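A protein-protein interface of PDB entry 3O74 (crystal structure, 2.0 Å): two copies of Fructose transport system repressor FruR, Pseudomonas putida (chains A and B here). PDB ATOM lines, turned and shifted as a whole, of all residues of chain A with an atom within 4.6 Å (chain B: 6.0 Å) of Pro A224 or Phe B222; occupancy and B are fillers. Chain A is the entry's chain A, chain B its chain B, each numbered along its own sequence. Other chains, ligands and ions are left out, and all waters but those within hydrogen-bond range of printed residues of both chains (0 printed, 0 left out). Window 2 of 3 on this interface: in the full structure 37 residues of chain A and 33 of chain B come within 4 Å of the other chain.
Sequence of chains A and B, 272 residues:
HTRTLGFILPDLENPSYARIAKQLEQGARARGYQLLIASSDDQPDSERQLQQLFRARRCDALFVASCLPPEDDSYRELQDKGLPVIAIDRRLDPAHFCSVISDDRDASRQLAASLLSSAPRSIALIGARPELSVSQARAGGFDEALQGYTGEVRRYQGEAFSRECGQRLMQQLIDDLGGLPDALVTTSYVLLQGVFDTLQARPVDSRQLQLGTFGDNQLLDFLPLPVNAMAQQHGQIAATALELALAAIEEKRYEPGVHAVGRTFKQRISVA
Phe A222 touches Leu B223, but with the chains exchanged Leu A223 does not touch Phe B222 (4.1 Å). Pro A224 touches Phe B222, but with the chains exchanged Phe A222 does not touch Pro B224 (4.5 Å).
Of the 8 printed residues of chain B, 4 touch a printed residue of chain A. Printed residues of chain B that touch a printed residue of chain A: Gln B218, Leu B219, Phe B222 and Leu B223. Hydrophobic or aromatic side chains of chain B that line the printed part of chain A: Leu B219, Phe B222 and Leu B223. Of the 8 printed residues of chain A, 4 touch a printed residue of chain B. Among the printed residues, 6 pairs touch across the chains. Among the printed residues, no Asp or Glu carboxylate lies within 4 Å of a Lys or Arg side-chain nitrogen of the other chain.
Of the printed residues of chain B, Phe A196 touches Gln B218, Leu B219 and Phe B222. Of the printed residues of chain B, Gln A200 touches Phe B222. Of the printed residues of chain B, Phe A222 touches Leu B223. Printed residues of chain B within 4 Å of Pro A224: Phe B222 (3.7 Å). Printed residues of chain A within 4 Å of Gln B218: Phe A196 (3.3 Å). Of the printed residues of chain A, Leu B219 touches Phe A196. Of the printed residues of chain A, Phe B222 touches Phe A196 (3.3 Å), Gln A200 (3.7 Å) and Pro A224 (3.7 Å). Pro B224 touches none of the printed residues of chain A. The nearest residue of chain A that does not touch Phe B222 is Leu A223 (4.1 Å).
Among the printed residues, merely in contact across the chains: Phe A196 with Gln B218, Phe A196 with Leu B219, Phe A196 with Phe B222, Gln A200 with Phe B222, Phe A222 with Leu B223 and Pro A224 with Phe B222.
O of Gln A200 sits at hydrogen-bond distance from NH2 of Arg A207 (3.2 Å).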
ATOM      1  N   PHE A 196      -5.372   9.648  -1.721  1.00  0.00           N
ATOM      2  CA  PHE A 196      -6.631   9.751  -2.457  1.00  0.00           C
ATOM      3  C   PHE A 196      -7.178  11.184  -2.471  1.00  0.00           C
ATOM      4  O   PHE A 196      -7.794  11.611  -3.449  1.00  0.00           O
ATOM      5  CB  PHE A 196      -7.684   8.799  -1.877  1.00  0.00           C
ATOM      6  CG  PHE A 196      -7.491   7.354  -2.264  1.00  0.00           C
ATOM      7  CD1 PHE A 196      -7.765   6.340  -1.360  1.00  0.00           C
ATOM      8  CD2 PHE A 196      -7.046   7.010  -3.530  1.00  0.00           C
ATOM      9  CE1 PHE A 196      -7.598   5.013  -1.714  1.00  0.00           C
ATOM     10  CE2 PHE A 196      -6.875   5.679  -3.890  1.00  0.00           C
ATOM     11  CZ  PHE A 196      -7.152   4.682  -2.980  1.00  0.00           C
ATOM     12  N   GLN A 200      -7.865  13.252  -5.927  1.00  0.00           N
ATOM     13  CA  GLN A 200      -9.233  13.710  -6.124  1.00  0.00           C
ATOM     14  C   GLN A 200      -9.270  15.116  -6.721  1.00  0.00           C
ATOM     15  O   GLN A 200     -10.191  15.468  -7.458  1.00  0.00           O
ATOM     16  CB  GLN A 200      -9.979  13.665  -4.790  1.00  0.00           C
ATOM     17  CG  GLN A 200     -11.385  13.117  -4.880  1.00  0.00           C
ATOM     18  CD  GLN A 200     -12.366  14.144  -5.382  1.00  0.00           C
ATOM     19  OE1 GLN A 200     -12.569  15.184  -4.753  1.00  0.00           O
ATOM     20  NE2 GLN A 200     -12.987  13.861  -6.521  1.00  0.00           N
ATOM     21  N   ARG A 207      -5.545  10.376 -12.841  1.00  0.00           N
ATOM     22  CA  ARG A 207      -5.479   9.697 -11.549  1.00  0.00           C
ATOM     23  C   ARG A 207      -4.935   8.272 -11.644  1.00  0.00           C
ATOM     24  O   ARG A 207      -4.904   7.548 -10.651  1.00  0.00           O
ATOM     25  CB  ARG A 207      -6.851   9.689 -10.871  1.00  0.00           C
ATOM     26  CG  ARG A 207      -7.475  11.064 -10.706  1.00  0.00           C
ATOM     27  CD  ARG A 207      -8.888  10.953 -10.167  1.00  0.00           C
ATOM     28  NE  ARG A 207      -9.566  12.244 -10.141  1.00  0.00           N
ATOM     29  CZ  ARG A 207     -10.850  12.407  -9.841  1.00  0.00           C
ATOM     30  NH1 ARG A 207     -11.601  11.357  -9.541  1.00  0.00           N
ATOM     31  NH2 ARG A 207     -11.383  13.621  -9.845  1.00  0.00           N
ATOM     32  N   PHE A 222     -14.525  -1.649  -5.846  1.00  0.00           N
ATOM     33  CA  PHE A 222     -15.418  -0.970  -6.780  1.00  0.00           C
ATOM     34  C   PHE A 222     -14.760   0.152  -7.593  1.00  0.00           C
ATOM     35  O   PHE A 222     -15.315   0.595  -8.602  1.00  0.00           O
ATOM     36  CB  PHE A 222     -16.657  -0.442  -6.048  1.00  0.00           C
ATOM     37  CG  PHE A 222     -17.238  -1.417  -5.058  1.00  0.00           C
ATOM     38  CD1 PHE A 222     -17.501  -1.026  -3.755  1.00  0.00           C
ATOM     39  CD2 PHE A 222     -17.505  -2.726  -5.422  1.00  0.00           C
ATOM     40  CE1 PHE A 222     -18.031  -1.920  -2.837  1.00  0.00           C
ATOM     41  CE2 PHE A 222     -18.032  -3.625  -4.506  1.00  0.00           C
ATOM     42  CZ  PHE A 222     -18.296  -3.220  -3.214  1.00  0.00           C
ATOM     43  N   LEU A 223     -13.586   0.609  -7.161  1.00  0.00           N
ATOM     44  CA  LEU A 223     -12.897   1.693  -7.857  1.00  0.00           C
ATOM     45  C   LEU A 223     -12.468   1.292  -9.260  1.00  0.00           C
ATOM     46  O   LEU A 223     -11.967   0.185  -9.474  1.00  0.00           O
ATOM     47  CB  LEU A 223     -11.665   2.168  -7.079  1.00  0.00           C
ATOM     48  CG  LEU A 223     -11.855   3.026  -5.829  1.00  0.00           C
ATOM     49  CD1 LEU A 223     -12.017   2.145  -4.619  1.00  0.00           C
ATOM     50  CD2 LEU A 223     -10.667   3.953  -5.635  1.00  0.00           C
ATOM     51  N   PRO A 224     -12.642   2.208 -10.224  1.00  0.00           N
ATOM     52  CA  PRO A 224     -12.112   1.983 -11.571  1.00  0.00           C
ATOM     53  C   PRO A 224     -10.602   1.774 -11.501  1.00  0.00           C
ATOM     54  O   PRO A 224     -10.009   1.217 -12.426  1.00  0.00           O
ATOM     55  CB  PRO A 224     -12.435   3.292 -12.302  1.00  0.00           C
ATOM     56  CG  PRO A 224     -12.627   4.302 -11.218  1.00  0.00           C
ATOM     57  CD  PRO A 224     -13.238   3.546 -10.081  1.00  0.00           C
ATOM     58  N   LEU A 225      -9.994   2.227 -10.407  1.00  0.00           N
ATOM     59  CA  LEU A 225      -8.564   2.043 -10.183  1.00  0.00           C
ATOM     60  C   LEU A 225      -8.303   0.910  -9.195  1.00  0.00           C
ATOM     61  O   LEU A 225      -8.612   1.029  -8.011  1.00  0.00           O
ATOM     62  CB  LEU A 225      -7.930   3.332  -9.661  1.00  0.00           C
ATOM     63  CG  LEU A 225      -6.419   3.257  -9.426  1.00  0.00           C
ATOM     64  CD1 LEU A 225      -5.676   3.187 -10.755  1.00  0.00           C
ATOM     65  CD2 LEU A 225      -5.939   4.440  -8.604  1.00  0.00           C
ATOM     66  N   PRO A 226      -7.718  -0.193  -9.680  1.00  0.00           N
ATOM     67  CA  PRO A 226      -7.409  -1.332  -8.808  1.00  0.00           C
ATOM     68  C   PRO A 226      -6.262  -1.015  -7.852  1.00  0.00           C
ATOM     69  O   PRO A 226      -5.273  -0.406  -8.259  1.00  0.00           O
ATOM     70  CB  PRO A 226      -6.989  -2.421  -9.799  1.00  0.00           C
ATOM     71  CG  PRO A 226      -6.469  -1.670 -10.986  1.00  0.00           C
ATOM     72  CD  PRO A 226      -7.278  -0.408 -11.070  1.00  0.00           C
ATOM     73  N   GLN B 218     -15.111   8.456   2.131  1.00  0.00           N
ATOM     74  CA  GLN B 218     -14.235   9.129   1.186  1.00  0.00           C
ATOM     75  C   GLN B 218     -14.302   8.519  -0.210  1.00  0.00           C
ATOM     76  O   GLN B 218     -14.339   9.237  -1.209  1.00  0.00           O
ATOM     77  CB  GLN B 218     -12.797   9.075   1.702  1.00  0.00           C
ATOM     78  CG  GLN B 218     -11.766   9.540   0.705  1.00  0.00           C
ATOM     79  CD  GLN B 218     -10.351   9.274   1.175  1.00  0.00           C
ATOM     80  OE1 GLN B 218     -10.111   8.388   1.993  1.00  0.00           O
ATOM     81  NE2 GLN B 218      -9.405  10.042   0.657  1.00  0.00           N
ATOM     82  N   LEU B 219     -14.318   7.194  -0.278  1.00  0.00           N
ATOM     83  CA  LEU B 219     -14.225   6.514  -1.565  1.00  0.00           C
ATOM     84  C   LEU B 219     -15.488   6.684  -2.416  1.00  0.00           C
ATOM     85  O   LEU B 219     -15.489   6.361  -3.604  1.00  0.00           O
ATOM     86  CB  LEU B 219     -13.840   5.039  -1.386  1.00  0.00           C
ATOM     87  CG  LEU B 219     -12.562   4.784  -0.580  1.00  0.00           C
ATOM     88  CD1 LEU B 219     -12.063   3.360  -0.776  1.00  0.00           C
ATOM     89  CD2 LEU B 219     -11.479   5.776  -0.968  1.00  0.00           C
ATOM     90  N   LEU B 220     -16.550   7.208  -1.813  1.00  0.00           N
ATOM     91  CA  LEU B 220     -17.750   7.568  -2.561  1.00  0.00           C
ATOM     92  C   LEU B 220     -17.437   8.631  -3.616  1.00  0.00           C
ATOM     93  O   LEU B 220     -18.153   8.763  -4.609  1.00  0.00           O
ATOM     94  CB  LEU B 220     -18.843   8.078  -1.619  1.00  0.00           C
ATOM     95  CG  LEU B 220     -20.072   7.192  -1.401  1.00  0.00           C
ATOM     96  CD1 LEU B 220     -19.669   5.742  -1.190  1.00  0.00           C
ATOM     97  CD2 LEU B 220     -20.909   7.703  -0.233  1.00  0.00           C
ATOM     98  N   ASP B 221     -16.369   9.392  -3.393  1.00  0.00           N
ATOM     99  CA  ASP B 221     -15.952  10.426  -4.334  1.00  0.00           C
ATOM    100  C   ASP B 221     -15.433   9.821  -5.637  1.00  0.00           C
ATOM    101  O   ASP B 221     -15.382  10.496  -6.662  1.00  0.00           O
ATOM    102  CB  ASP B 221     -14.873  11.320  -3.715  1.00  0.00           C
ATOM    103  CG  ASP B 221     -15.430  12.288  -2.683  1.00  0.00           C
ATOM    104  OD1 ASP B 221     -16.473  12.919  -2.951  1.00  0.00           O
ATOM    105  OD2 ASP B 221     -14.809  12.428  -1.608  1.00  0.00           O
ATOM    106  N   PHE B 222     -15.048   8.548  -5.583  1.00  0.00           N
ATOM    107  CA  PHE B 222     -14.449   7.866  -6.727  1.00  0.00           C
ATOM    108  C   PHE B 222     -15.404   6.878  -7.395  1.00  0.00           C
ATOM    109  O   PHE B 222     -15.085   6.308  -8.441  1.00  0.00           O
ATOM    110  CB  PHE B 222     -13.179   7.131  -6.299  1.00  0.00           C
ATOM    111  CG  PHE B 222     -12.115   8.029  -5.737  1.00  0.00           C
ATOM    112  CD1 PHE B 222     -11.103   8.514  -6.548  1.00  0.00           C
ATOM    113  CD2 PHE B 222     -12.123   8.384  -4.400  1.00  0.00           C
ATOM    114  CE1 PHE B 222     -10.117   9.340  -6.037  1.00  0.00           C
ATOM    115  CE2 PHE B 222     -11.143   9.209  -3.882  1.00  0.00           C
ATOM    116  CZ  PHE B 222     -10.139   9.688  -4.703  1.00  0.00           C
ATOM    117  N   LEU B 223     -16.559   6.660  -6.775  1.00  0.00           N
ATOM    118  CA  LEU B 223     -17.579   5.787  -7.348  1.00  0.00           C
ATOM    119  C   LEU B 223     -18.170   6.398  -8.608  1.00  0.00           C
ATOM    120  O   LEU B 223     -18.510   7.581  -8.624  1.00  0.00           O
ATOM    121  CB  LEU B 223     -18.710   5.535  -6.348  1.00  0.00           C
ATOM    122  CG  LEU B 223     -18.607   4.346  -5.398  1.00  0.00           C
ATOM    123  CD1 LEU B 223     -19.974   4.071  -4.800  1.00  0.00           C
ATOM    124  CD2 LEU B 223     -18.091   3.123  -6.129  1.00  0.00           C
ATOM    125  N   PRO B 224     -18.297   5.591  -9.671  1.00  0.00           N
ATOM    126  CA  PRO B 224     -19.012   6.023 -10.876  1.00  0.00           C
ATOM    127  C   PRO B 224     -20.478   6.257 -10.535  1.00  0.00           C
ATOM    128  O   PRO B 224     -21.112   7.175 -11.053  1.00  0.00           O
ATOM    129  CB  PRO B 224     -18.879   4.820 -11.814  1.00  0.00           C
ATOM    130  CG  PRO B 224     -17.705   4.060 -11.305  1.00  0.00           C
ATOM    131  CD  PRO B 224     -17.723   4.245  -9.824  1.00  0.00           C
ATOM    132  N   ARG B 268     -23.712  14.248  -4.392  1.00  0.00           N
ATOM    133  CA  ARG B 268     -22.851  13.803  -5.471  1.00  0.00           C
ATOM    134  C   ARG B 268     -23.686  13.563  -6.721  1.00  0.00           C
ATOM    135  O   ARG B 268     -23.151  13.399  -7.815  1.00  0.00           O
ATOM    136  CB  ARG B 268     -22.105  12.538  -5.055  1.00  0.00           C
ATOM    137  CG  ARG B 268     -21.266  12.734  -3.808  1.00  0.00           C
ATOM    138  CD  ARG B 268     -20.739  11.419  -3.281  1.00  0.00           C
ATOM    139  NE  ARG B 268     -20.387  11.514  -1.868  1.00  0.00           N
ATOM    140  CZ  ARG B 268     -19.150  11.414  -1.403  1.00  0.00           C
ATOM    141  NH1 ARG B 268     -18.147  11.204  -2.240  1.00  0.00           N
ATOM    142  NH2 ARG B 268     -18.912  11.514  -0.105  1.00  0.00           N
